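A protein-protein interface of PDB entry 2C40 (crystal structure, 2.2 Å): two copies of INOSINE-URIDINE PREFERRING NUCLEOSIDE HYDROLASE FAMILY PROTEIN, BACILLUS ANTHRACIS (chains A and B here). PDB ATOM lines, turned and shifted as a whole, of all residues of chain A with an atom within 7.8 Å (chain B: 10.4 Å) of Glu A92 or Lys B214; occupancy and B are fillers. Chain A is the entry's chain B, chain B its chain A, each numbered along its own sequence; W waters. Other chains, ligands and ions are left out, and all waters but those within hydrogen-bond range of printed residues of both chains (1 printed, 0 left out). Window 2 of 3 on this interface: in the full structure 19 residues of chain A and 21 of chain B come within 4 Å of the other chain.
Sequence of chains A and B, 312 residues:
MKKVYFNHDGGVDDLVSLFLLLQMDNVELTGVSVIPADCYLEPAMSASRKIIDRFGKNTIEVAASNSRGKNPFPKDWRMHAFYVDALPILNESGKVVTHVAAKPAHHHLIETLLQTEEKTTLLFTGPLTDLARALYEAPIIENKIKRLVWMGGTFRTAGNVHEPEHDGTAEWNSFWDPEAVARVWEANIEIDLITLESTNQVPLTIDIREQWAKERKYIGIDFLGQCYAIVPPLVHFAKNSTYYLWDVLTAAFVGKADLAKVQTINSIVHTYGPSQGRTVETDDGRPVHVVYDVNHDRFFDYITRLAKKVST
Of the 20 printed residues of chain B, 6 touch a printed residue of chain A. Printed residues of chain B that touch a printed residue of chain A: Ala B213, Lys B214, Arg B216, Asp B222, Gly B225 and Gln B226. Hydrophobic or aromatic side chains of chain B within 4 Å of the printed part of chain A: Ala B213. Of the 12 printed residues of chain A, 6 touch a printed residue of chain B. Among the printed residues, Asp or Glu carboxylates within 4 Å of a Lys or Arg side-chain nitrogen of the other chain: Glu A92 with Arg B216 (3.1 Å).
OE1 of Glu A92 lies within salt-bridge range of NE of Arg B216 (3.1 Å).
Of chain B, only Ala B213, Lys B214 and Arg B216 come within 4 Å of Glu A92. Lys B214 touches one residue of chain A. Asn A91 touches just one residue of chain B: Ala B213. No residue of chain B comes within 4 Å of Ser A93. Printed residues of chain A within 4 Å of Ala B213: Pro A88 (3.97 Å), Asn A91 (3.6 Å) and Glu A92 (3.4 Å). Printed residues of chain A within 4 Å of Gln B226: Pro A88 (3.5 Å). Printed residues of chain B within 4 Å of Pro A88: Ala B213 (3.97 Å), Arg B216 (3.6 Å), Asp B222 (3.6 Å), Gly B225 (3.4 Å) and Gln B226 (3.5 Å). Printed residues of chain A within 4 Å of Gly B225: Pro A88. Printed residues of chain A within 4 Å of Asp B222: Pro A88 (3.6 Å). The nearest printed residue of chain A that does not touch Asp B222 is Ile A89 (4.8 Å).
1 position is printed for both chains. Of the 12 pairs that touch across the chains among the printed residues, none has its exchanged pair printed and touching as well.
O of Leu A87 lies within hydrogen-bond range of ND2 of Asn A91 (2.8 Å). NH1 of Arg A54 sits close to O of Ile A89, 3.5 Å away. The guanidinium group (NH1) of Arg B216 lies within salt-bridge range of the side-chain carboxylate (OD2) of Asp B222 (3.4 Å). NZ of Lys A50 sits at hydrogen-bond distance from OD1 of Asn A91, 2.6 Å away. The guanidinium group (NH1) of Arg A54 lies within salt-bridge range of the side-chain carboxylate (OE1) of Glu A92 (3.2 Å). The side-chain amide nitrogen of Gln B226 sits at hydrogen-bond distance from the side-chain carboxylate of Asp B222, 3.1 Å away.
Water W1 bridges the backbone NH of Ile A89 and the side-chain carboxylate of Asp B222.
Arg A54 touches Arg B216 (NH1 to NH2, 3.97 Å). Pro A88 touches Ala B213 (O to CB, 3.97 Å). Pro A88 touches Arg B216 (C to CD, 3.6 Å). Pro A88 touches Gly B225. Gln B226 touches Pro A88 (N to CG, 3.5 Å). Ile A89 touches Arg B216. Asn A91 touches Ala B213 (CB to CB, 3.6 Å). O of Ala B213 touches CG of Glu A92, at 3.4 Å. Glu A92 touches Lys B214. Ile A219 touches Arg B216 (CD1 to NH2, 3.2 Å).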
ATOM      1  N   LYS A  50     -12.218   4.733  21.812  1.00  0.00           N
ATOM      2  CA  LYS A  50     -11.733   5.032  20.458  1.00  0.00           C
ATOM      3  C   LYS A  50     -12.394   4.163  19.389  1.00  0.00           C
ATOM      4  O   LYS A  50     -12.589   4.581  18.261  1.00  0.00           O
ATOM      5  CB  LYS A  50     -10.232   4.831  20.406  1.00  0.00           C
ATOM      6  CG  LYS A  50      -9.464   5.773  21.259  1.00  0.00           C
ATOM      7  CD  LYS A  50      -7.976   5.394  21.293  1.00  0.00           C
ATOM      8  CE  LYS A  50      -7.125   6.408  22.009  1.00  0.00           C
ATOM      9  NZ  LYS A  50      -5.738   5.956  22.152  1.00  0.00           N
ATOM     10  N   ARG A  54     -14.614   5.669  16.448  1.00  0.00           N
ATOM     11  CA  ARG A  54     -14.202   5.317  15.094  1.00  0.00           C
ATOM     12  C   ARG A  54     -15.201   4.426  14.342  1.00  0.00           C
ATOM     13  O   ARG A  54     -15.428   4.606  13.151  1.00  0.00           O
ATOM     14  CB  ARG A  54     -12.846   4.616  15.182  1.00  0.00           C
ATOM     15  CG  ARG A  54     -12.253   4.216  13.862  1.00  0.00           C
ATOM     16  CD  ARG A  54     -11.850   5.421  13.084  1.00  0.00           C
ATOM     17  NE  ARG A  54     -12.078   5.225  11.667  1.00  0.00           N
ATOM     18  CZ  ARG A  54     -11.156   5.278  10.714  1.00  0.00           C
ATOM     19  NH1 ARG A  54      -9.860   5.562  10.983  1.00  0.00           N
ATOM     20  NH2 ARG A  54     -11.560   5.073   9.460  1.00  0.00           N
ATOM     21  N   LEU A  87      -2.851   1.676  18.370  1.00  0.00           N
ATOM     22  CA  LEU A  87      -2.898   1.507  16.896  1.00  0.00           C
ATOM     23  C   LEU A  87      -3.267   2.822  16.175  1.00  0.00           C
ATOM     24  O   LEU A  87      -4.272   3.486  16.536  1.00  0.00           O
ATOM     25  CB  LEU A  87      -3.872   0.412  16.425  1.00  0.00           C
ATOM     26  CG  LEU A  87      -3.523  -1.019  16.856  1.00  0.00           C
ATOM     27  CD1 LEU A  87      -4.667  -1.956  16.492  1.00  0.00           C
ATOM     28  CD2 LEU A  87      -2.157  -1.466  16.322  1.00  0.00           C
ATOM     29  N   PRO A  88      -2.493   3.183  15.139  1.00  0.00           N
ATOM     30  CA  PRO A  88      -2.775   4.428  14.426  1.00  0.00           C
ATOM     31  C   PRO A  88      -4.244   4.613  14.037  1.00  0.00           C
ATOM     32  O   PRO A  88      -4.808   5.679  14.266  1.00  0.00           O
ATOM     33  CB  PRO A  88      -1.885   4.332  13.185  1.00  0.00           C
ATOM     34  CG  PRO A  88      -0.722   3.504  13.626  1.00  0.00           C
ATOM     35  CD  PRO A  88      -1.331   2.483  14.573  1.00  0.00           C
ATOM     36  N   ILE A  89      -4.866   3.575  13.481  1.00  0.00           N
ATOM     37  CA  ILE A  89      -6.309   3.616  13.122  1.00  0.00           C
ATOM     38  C   ILE A  89      -7.186   4.235  14.222  1.00  0.00           C
ATOM     39  O   ILE A  89      -8.151   5.001  13.949  1.00  0.00           O
ATOM     40  CB  ILE A  89      -6.820   2.195  12.816  1.00  0.00           C
ATOM     41  CG1 ILE A  89      -8.334   2.143  12.551  1.00  0.00           C
ATOM     42  CG2 ILE A  89      -6.530   1.246  13.975  1.00  0.00           C
ATOM     43  CD1 ILE A  89      -8.672   2.393  11.096  1.00  0.00           C
ATOM     44  N   LEU A  90      -6.867   3.890  15.469  1.00  0.00           N
ATOM     45  CA  LEU A  90      -7.672   4.299  16.586  1.00  0.00           C
ATOM     46  C   LEU A  90      -7.272   5.662  17.162  1.00  0.00           C
ATOM     47  O   LEU A  90      -8.021   6.212  17.959  1.00  0.00           O
ATOM     48  CB  LEU A  90      -7.690   3.229  17.703  1.00  0.00           C
ATOM     49  CG  LEU A  90      -8.421   1.919  17.441  1.00  0.00           C
ATOM     50  CD1 LEU A  90      -8.372   1.151  18.717  1.00  0.00           C
ATOM     51  CD2 LEU A  90      -9.882   2.157  16.943  1.00  0.00           C
ATOM     52  N   ASN A  91      -6.127   6.190  16.736  1.00  0.00           N
ATOM     53  CA  ASN A  91      -5.595   7.483  17.178  1.00  0.00           C
ATOM     54  C   ASN A  91      -5.615   8.579  16.109  1.00  0.00           C
ATOM     55  O   ASN A  91      -5.310   9.730  16.390  1.00  0.00           O
ATOM     56  CB  ASN A  91      -4.184   7.250  17.701  1.00  0.00           C
ATOM     57  CG  ASN A  91      -4.201   6.409  18.954  1.00  0.00           C
ATOM     58  OD1 ASN A  91      -4.474   6.921  20.039  1.00  0.00           O
ATOM     59  ND2 ASN A  91      -4.024   5.100  18.802  1.00  0.00           N
ATOM     60  N   GLU A  92      -6.011   8.212  14.893  1.00  0.00           N
ATOM     61  CA  GLU A  92      -5.952   9.112  13.742  1.00  0.00           C
ATOM     62  C   GLU A  92      -6.757  10.403  13.972  1.00  0.00           C
ATOM     63  O   GLU A  92      -6.382  11.463  13.492  1.00  0.00           O
ATOM     64  CB  GLU A  92      -6.466   8.401  12.481  1.00  0.00           C
ATOM     65  CG  GLU A  92      -6.327   9.215  11.204  1.00  0.00           C
ATOM     66  CD  GLU A  92      -6.710   8.430   9.945  1.00  0.00           C
ATOM     67  OE1 GLU A  92      -7.369   7.370  10.076  1.00  0.00           O
ATOM     68  OE2 GLU A  92      -6.356   8.887   8.817  1.00  0.00           O
ATOM     69  N   SER A  93      -7.853  10.308  14.704  1.00  0.00           N
ATOM     70  CA  SER A  93      -8.743  11.455  14.933  1.00  0.00           C
ATOM     71  C   SER A  93      -8.219  12.438  15.979  1.00  0.00           C
ATOM     72  O   SER A  93      -8.684  13.558  16.036  1.00  0.00           O
ATOM     73  CB  SER A  93     -10.126  10.968  15.364  1.00  0.00           C
ATOM     74  OG  SER A  93     -10.120  10.665  16.755  1.00  0.00           O
ATOM     75  N   GLY A  94      -7.274  12.004  16.814  1.00  0.00           N
ATOM     76  CA  GLY A  94      -6.601  12.877  17.755  1.00  0.00           C
ATOM     77  C   GLY A  94      -7.477  13.378  18.876  1.00  0.00           C
ATOM     78  O   GLY A  94      -7.150  14.363  19.517  1.00  0.00           O
ATOM     79  N   LYS A  95      -8.606  12.712  19.088  1.00  0.00           N
ATOM     80  CA  LYS A  95      -9.586  13.107  20.091  1.00  0.00           C
ATOM     81  C   LYS A  95     -10.302  11.859  20.526  1.00  0.00           C
ATOM     82  O   LYS A  95     -10.477  10.946  19.718  1.00  0.00           O
ATOM     83  CB  LYS A  95     -10.645  14.050  19.495  1.00  0.00           C
ATOM     84  N   ILE A 219     -10.899  -1.401   5.648  1.00  0.00           N
ATOM     85  CA  ILE A 219     -10.247  -0.860   6.835  1.00  0.00           C
ATOM     86  C   ILE A 219     -10.602  -1.617   8.142  1.00  0.00           C
ATOM     87  O   ILE A 219      -9.775  -1.697   9.066  1.00  0.00           O
ATOM     88  CB  ILE A 219     -10.542   0.639   6.957  1.00  0.00           C
ATOM     89  CG1 ILE A 219      -9.631   1.289   7.981  1.00  0.00           C
ATOM     90  CG2 ILE A 219     -11.991   0.895   7.348  1.00  0.00           C
ATOM     91  CD1 ILE A 219      -9.943   2.760   8.133  1.00  0.00           C
ATOM     92  N   ILE B 206       4.436  10.613  23.265  1.00  0.00           N
ATOM     93  CA  ILE B 206       3.026  10.454  22.891  1.00  0.00           C
ATOM     94  C   ILE B 206       2.623  11.495  21.815  1.00  0.00           C
ATOM     95  O   ILE B 206       1.963  11.152  20.838  1.00  0.00           O
ATOM     96  CB  ILE B 206       2.070  10.545  24.170  1.00  0.00           C
ATOM     97  CG1 ILE B 206       2.225   9.325  25.086  1.00  0.00           C
ATOM     98  CG2 ILE B 206       0.594  10.743  23.779  1.00  0.00           C
ATOM     99  CD1 ILE B 206       1.794   9.631  26.606  1.00  0.00           C
ATOM    100  N   ASP B 207       3.025  12.756  22.011  1.00  0.00           N
ATOM    101  CA  ASP B 207       2.796  13.817  21.033  1.00  0.00           C
ATOM    102  C   ASP B 207       3.310  13.480  19.642  1.00  0.00           C
ATOM    103  O   ASP B 207       2.730  13.889  18.655  1.00  0.00           O
ATOM    104  CB  ASP B 207       3.428  15.138  21.495  1.00  0.00           C
ATOM    105  N   ILE B 208       4.366  12.693  19.560  1.00  0.00           N
ATOM    106  CA  ILE B 208       4.934  12.290  18.260  1.00  0.00           C
ATOM    107  C   ILE B 208       4.173  11.113  17.677  1.00  0.00           C
ATOM    108  O   ILE B 208       3.908  11.077  16.481  1.00  0.00           O
ATOM    109  CB  ILE B 208       6.473  12.017  18.365  1.00  0.00           C
ATOM    110  CG1 ILE B 208       7.197  13.357  18.512  1.00  0.00           C
ATOM    111  CG2 ILE B 208       7.001  11.259  17.171  1.00  0.00           C
ATOM    112  CD1 ILE B 208       8.606  13.251  18.966  1.00  0.00           C
ATOM    113  N   ARG B 209       3.845  10.149  18.533  1.00  0.00           N
ATOM    114  CA  ARG B 209       2.993   9.015  18.147  1.00  0.00           C
ATOM    115  C   ARG B 209       1.658   9.521  17.633  1.00  0.00           C
ATOM    116  O   ARG B 209       1.202   9.066  16.609  1.00  0.00           O
ATOM    117  CB  ARG B 209       2.796   8.069  19.324  1.00  0.00           C
ATOM    118  CG  ARG B 209       4.068   7.308  19.801  1.00  0.00           C
ATOM    119  CD  ARG B 209       3.850   6.744  21.237  1.00  0.00           C
ATOM    120  NE  ARG B 209       5.055   6.138  21.789  1.00  0.00           N
ATOM    121  CZ  ARG B 209       5.386   4.842  21.703  1.00  0.00           C
ATOM    122  NH1 ARG B 209       4.567   3.941  21.111  1.00  0.00           N
ATOM    123  NH2 ARG B 209       6.561   4.430  22.222  1.00  0.00           N
ATOM    124  N   GLU B 210       1.047  10.471  18.324  1.00  0.00           N
ATOM    125  CA  GLU B 210      -0.228  11.000  17.884  1.00  0.00           C
ATOM    126  C   GLU B 210      -0.176  11.737  16.564  1.00  0.00           C
ATOM    127  O   GLU B 210      -1.124  11.666  15.810  1.00  0.00           O
ATOM    128  CB  GLU B 210      -0.836  11.957  18.908  1.00  0.00           C
ATOM    129  CG  GLU B 210      -1.249  11.259  20.174  1.00  0.00           C
ATOM    130  CD  GLU B 210      -1.735  12.200  21.262  1.00  0.00           C
ATOM    131  OE1 GLU B 210      -2.368  11.663  22.210  1.00  0.00           O
ATOM    132  OE2 GLU B 210      -1.481  13.439  21.170  1.00  0.00           O
ATOM    133  N   GLN B 211       0.893  12.500  16.349  1.00  0.00           N
ATOM    134  CA  GLN B 211       1.101  13.258  15.126  1.00  0.00           C
ATOM    135  C   GLN B 211       1.368  12.331  13.935  1.00  0.00           C
ATOM    136  O   GLN B 211       0.950  12.606  12.820  1.00  0.00           O
ATOM    137  CB  GLN B 211       2.256  14.250  15.292  1.00  0.00           C
ATOM    138  N   TRP B 212       2.015  11.205  14.177  1.00  0.00           N
ATOM    139  CA  TRP B 212       2.068  10.130  13.180  1.00  0.00           C
ATOM    140  C   TRP B 212       0.716   9.505  12.856  1.00  0.00           C
ATOM    141  O   TRP B 212       0.420   9.300  11.680  1.00  0.00           O
ATOM    142  CB  TRP B 212       3.061   9.031  13.608  1.00  0.00           C
ATOM    143  CG  TRP B 212       4.524   9.434  13.410  1.00  0.00           C
ATOM    144  CD1 TRP B 212       4.979  10.403  12.589  1.00  0.00           C
ATOM    145  CD2 TRP B 212       5.682   8.833  14.000  1.00  0.00           C
ATOM    146  NE1 TRP B 212       6.322  10.453  12.631  1.00  0.00           N
ATOM    147  CE2 TRP B 212       6.794   9.512  13.494  1.00  0.00           C
ATOM    148  CE3 TRP B 212       5.880   7.792  14.892  1.00  0.00           C
ATOM    149  CZ2 TRP B 212       8.102   9.199  13.864  1.00  0.00           C
ATOM    150  CZ3 TRP B 212       7.157   7.482  15.274  1.00  0.00           C
ATOM    151  CH2 TRP B 212       8.260   8.180  14.769  1.00  0.00           C
ATOM    152  N   ALA B 213      -0.093   9.235  13.880  1.00  0.00           N
ATOM    153  CA  ALA B 213      -1.409   8.636  13.707  1.00  0.00           C
ATOM    154  C   ALA B 213      -2.312   9.524  12.832  1.00  0.00           C
ATOM    155  O   ALA B 213      -3.049   9.006  11.988  1.00  0.00           O
ATOM    156  CB  ALA B 213      -2.027   8.390  15.075  1.00  0.00           C
ATOM    157  N   LYS B 214      -2.257  10.844  13.044  1.00  0.00           N
ATOM    158  CA  LYS B 214      -3.001  11.826  12.239  1.00  0.00           C
ATOM    159  C   LYS B 214      -2.675  11.710  10.747  1.00  0.00           C
ATOM    160  O   LYS B 214      -3.508  12.009   9.905  1.00  0.00           O
ATOM    161  CB  LYS B 214      -2.752  13.276  12.741  1.00  0.00           C
ATOM    162  N   GLU B 215      -1.466  11.263  10.417  1.00  0.00           N
ATOM    163  CA  GLU B 215      -1.051  11.141   9.010  1.00  0.00           C
ATOM    164  C   GLU B 215      -0.927   9.712   8.533  1.00  0.00           C
ATOM    165  O   GLU B 215      -0.147   9.394   7.633  1.00  0.00           O
ATOM    166  CB  GLU B 215       0.257  11.915   8.766  1.00  0.00           C
ATOM    167  CG  GLU B 215       0.078  13.386   9.078  1.00  0.00           C
ATOM    168  CD  GLU B 215       1.146  14.229   8.480  1.00  0.00           C
ATOM    169  OE1 GLU B 215       2.313  13.828   8.597  1.00  0.00           O
ATOM    170  OE2 GLU B 215       0.811  15.299   7.917  1.00  0.00           O
ATOM    171  N   ARG B 216      -1.730   8.863   9.146  1.00  0.00           N
ATOM    172  CA  ARG B 216      -1.892   7.462   8.788  1.00  0.00           C
ATOM    173  C   ARG B 216      -2.187   7.258   7.289  1.00  0.00           C
ATOM    174  O   ARG B 216      -1.990   6.159   6.765  1.00  0.00           O
ATOM    175  CB  ARG B 216      -3.069   6.871   9.628  1.00  0.00           C
ATOM    176  CG  ARG B 216      -3.142   5.376   9.551  1.00  0.00           C
ATOM    177  CD  ARG B 216      -4.223   4.801  10.411  1.00  0.00           C
ATOM    178  NE  ARG B 216      -5.491   4.947   9.778  1.00  0.00           N
ATOM    179  CZ  ARG B 216      -5.959   4.144   8.831  1.00  0.00           C
ATOM    180  NH1 ARG B 216      -5.274   3.090   8.413  1.00  0.00           N
ATOM    181  NH2 ARG B 216      -7.152   4.392   8.327  1.00  0.00           N
ATOM    182  N   LYS B 217      -2.745   8.294   6.651  1.00  0.00           N
ATOM    183  CA  LYS B 217      -3.032   8.308   5.206  1.00  0.00           C
ATOM    184  C   LYS B 217      -1.801   7.936   4.378  1.00  0.00           C
ATOM    185  O   LYS B 217      -1.922   7.346   3.308  1.00  0.00           O
ATOM    186  CB  LYS B 217      -3.583   9.687   4.758  1.00  0.00           C
ATOM    187  CG  LYS B 217      -2.663  10.912   5.093  1.00  0.00           C
ATOM    188  CD  LYS B 217      -2.949  12.159   4.222  1.00  0.00           C
ATOM    189  CE  LYS B 217      -3.005  13.484   5.054  1.00  0.00           C
ATOM    190  NZ  LYS B 217      -1.699  13.967   5.668  1.00  0.00           N
ATOM    191  N   TYR B 218      -0.616   8.317   4.858  1.00  0.00           N
ATOM    192  CA  TYR B 218       0.627   7.846   4.268  1.00  0.00           C
ATOM    193  C   TYR B 218       0.895   6.448   4.786  1.00  0.00           C
ATOM    194  O   TYR B 218       0.993   6.247   6.005  1.00  0.00           O
ATOM    195  CB  TYR B 218       1.794   8.758   4.618  1.00  0.00           C
ATOM    196  CG  TYR B 218       1.673  10.111   3.974  1.00  0.00           C
ATOM    197  CD1 TYR B 218       1.050  11.156   4.647  1.00  0.00           C
ATOM    198  CD2 TYR B 218       2.182  10.344   2.702  1.00  0.00           C
ATOM    199  CE1 TYR B 218       0.925  12.381   4.084  1.00  0.00           C
ATOM    200  CE2 TYR B 218       2.071  11.594   2.129  1.00  0.00           C
ATOM    201  CZ  TYR B 218       1.428  12.600   2.829  1.00  0.00           C
ATOM    202  OH  TYR B 218       1.285  13.854   2.285  1.00  0.00           O
ATOM    203  N   ILE B 219       1.001   5.483   3.876  1.00  0.00           N
ATOM    204  CA  ILE B 219       1.068   4.080   4.295  1.00  0.00           C
ATOM    205  C   ILE B 219       2.343   3.776   5.117  1.00  0.00           C
ATOM    206  O   ILE B 219       2.307   2.940   6.024  1.00  0.00           O
ATOM    207  CB  ILE B 219       0.866   3.062   3.126  1.00  0.00           C
ATOM    208  CG1 ILE B 219       0.824   1.621   3.687  1.00  0.00           C
ATOM    209  CG2 ILE B 219       1.976   3.150   2.061  1.00  0.00           C
ATOM    210  CD1 ILE B 219       0.406   0.528   2.676  1.00  0.00           C
ATOM    211  N   ILE B 221       3.822   5.992   7.158  1.00  0.00           N
ATOM    212  CA  ILE B 221       3.544   6.562   8.475  1.00  0.00           C
ATOM    213  C   ILE B 221       2.640   5.571   9.273  1.00  0.00           C
ATOM    214  O   ILE B 221       2.930   5.268  10.425  1.00  0.00           O
ATOM    215  CB  ILE B 221       2.885   7.982   8.366  1.00  0.00           C
ATOM    216  CG1 ILE B 221       3.818   9.005   7.703  1.00  0.00           C
ATOM    217  CG2 ILE B 221       2.433   8.502   9.707  1.00  0.00           C
ATOM    218  CD1 ILE B 221       5.036   9.394   8.509  1.00  0.00           C
ATOM    219  N   ASP B 222       1.579   5.067   8.639  1.00  0.00           N
ATOM    220  CA  ASP B 222       0.693   4.066   9.232  1.00  0.00           C
ATOM    221  C   ASP B 222       1.545   2.849   9.642  1.00  0.00           C
ATOM    222  O   ASP B 222       1.419   2.355  10.762  1.00  0.00           O
ATOM    223  CB  ASP B 222      -0.372   3.688   8.220  1.00  0.00           C
ATOM    224  CG  ASP B 222      -1.449   2.762   8.767  1.00  0.00           C
ATOM    225  OD1 ASP B 222      -1.697   2.700  10.004  1.00  0.00           O
ATOM    226  OD2 ASP B 222      -2.087   2.110   7.913  1.00  0.00           O
ATOM    227  N   GLY B 225       3.625   3.741  12.727  1.00  0.00           N
ATOM    228  CA  GLY B 225       2.736   3.689  13.879  1.00  0.00           C
ATOM    229  C   GLY B 225       2.348   2.294  14.374  1.00  0.00           C
ATOM    230  O   GLY B 225       2.263   2.070  15.568  1.00  0.00           O
ATOM    231  N   GLN B 226       2.086   1.366  13.469  1.00  0.00           N
ATOM    232  CA  GLN B 226       1.802  -0.031  13.839  1.00  0.00           C
ATOM    233  C   GLN B 226       3.002  -0.632  14.549  1.00  0.00           C
ATOM    234  O   GLN B 226       2.871  -1.218  15.627  1.00  0.00           O
ATOM    235  CB  GLN B 226       1.441  -0.839  12.605  1.00  0.00           C
ATOM    236  CG  GLN B 226       0.036  -0.457  12.140  1.00  0.00           C
ATOM    237  CD  GLN B 226      -0.346  -1.060  10.818  1.00  0.00           C
ATOM    238  OE1 GLN B 226      -0.307  -2.258  10.650  1.00  0.00           O
ATOM    239  NE2 GLN B 226      -0.776  -0.223   9.890  1.00  0.00           N
ATOM    240  N   THR B 304      10.008  11.153   9.469  1.00  0.00           N
ATOM    241  CA  THR B 304       8.669  11.326   8.888  1.00  0.00           C
ATOM    242  C   THR B 304       8.728  11.663   7.382  1.00  0.00           C
ATOM    243  O   THR B 304       7.918  11.141   6.637  1.00  0.00           O
ATOM    244  CB  THR B 304       7.637  12.161   9.766  1.00  0.00           C
ATOM    245  OG1 THR B 304       7.000  13.230   9.023  1.00  0.00           O
ATOM    246  CG2 THR B 304       8.238  12.692  11.018  1.00  0.00           C
ATOM    247  N   LYS B 308       7.061   9.066   4.457  1.00  0.00           N
ATOM    248  CA  LYS B 308       6.116   9.572   3.463  1.00  0.00           C
ATOM    249  C   LYS B 308       6.521   9.294   2.004  1.00  0.00           C
ATOM    250  O   LYS B 308       5.684   9.445   1.127  1.00  0.00           O
ATOM    251  CB  LYS B 308       5.911  11.075   3.661  1.00  0.00           C
ATOM    252  CG  LYS B 308       5.161  11.407   4.946  1.00  0.00           C
ATOM    253  CD  LYS B 308       4.988  12.915   5.081  1.00  0.00           C
ATOM    254  CE  LYS B 308       4.074  13.256   6.224  1.00  0.00           C
ATOM    255  NZ  LYS B 308       3.779  14.710   6.276  1.00  0.00           N
HETATM  256  O   HOH W   1      -3.452   1.519  12.329  1.00  0.00           O
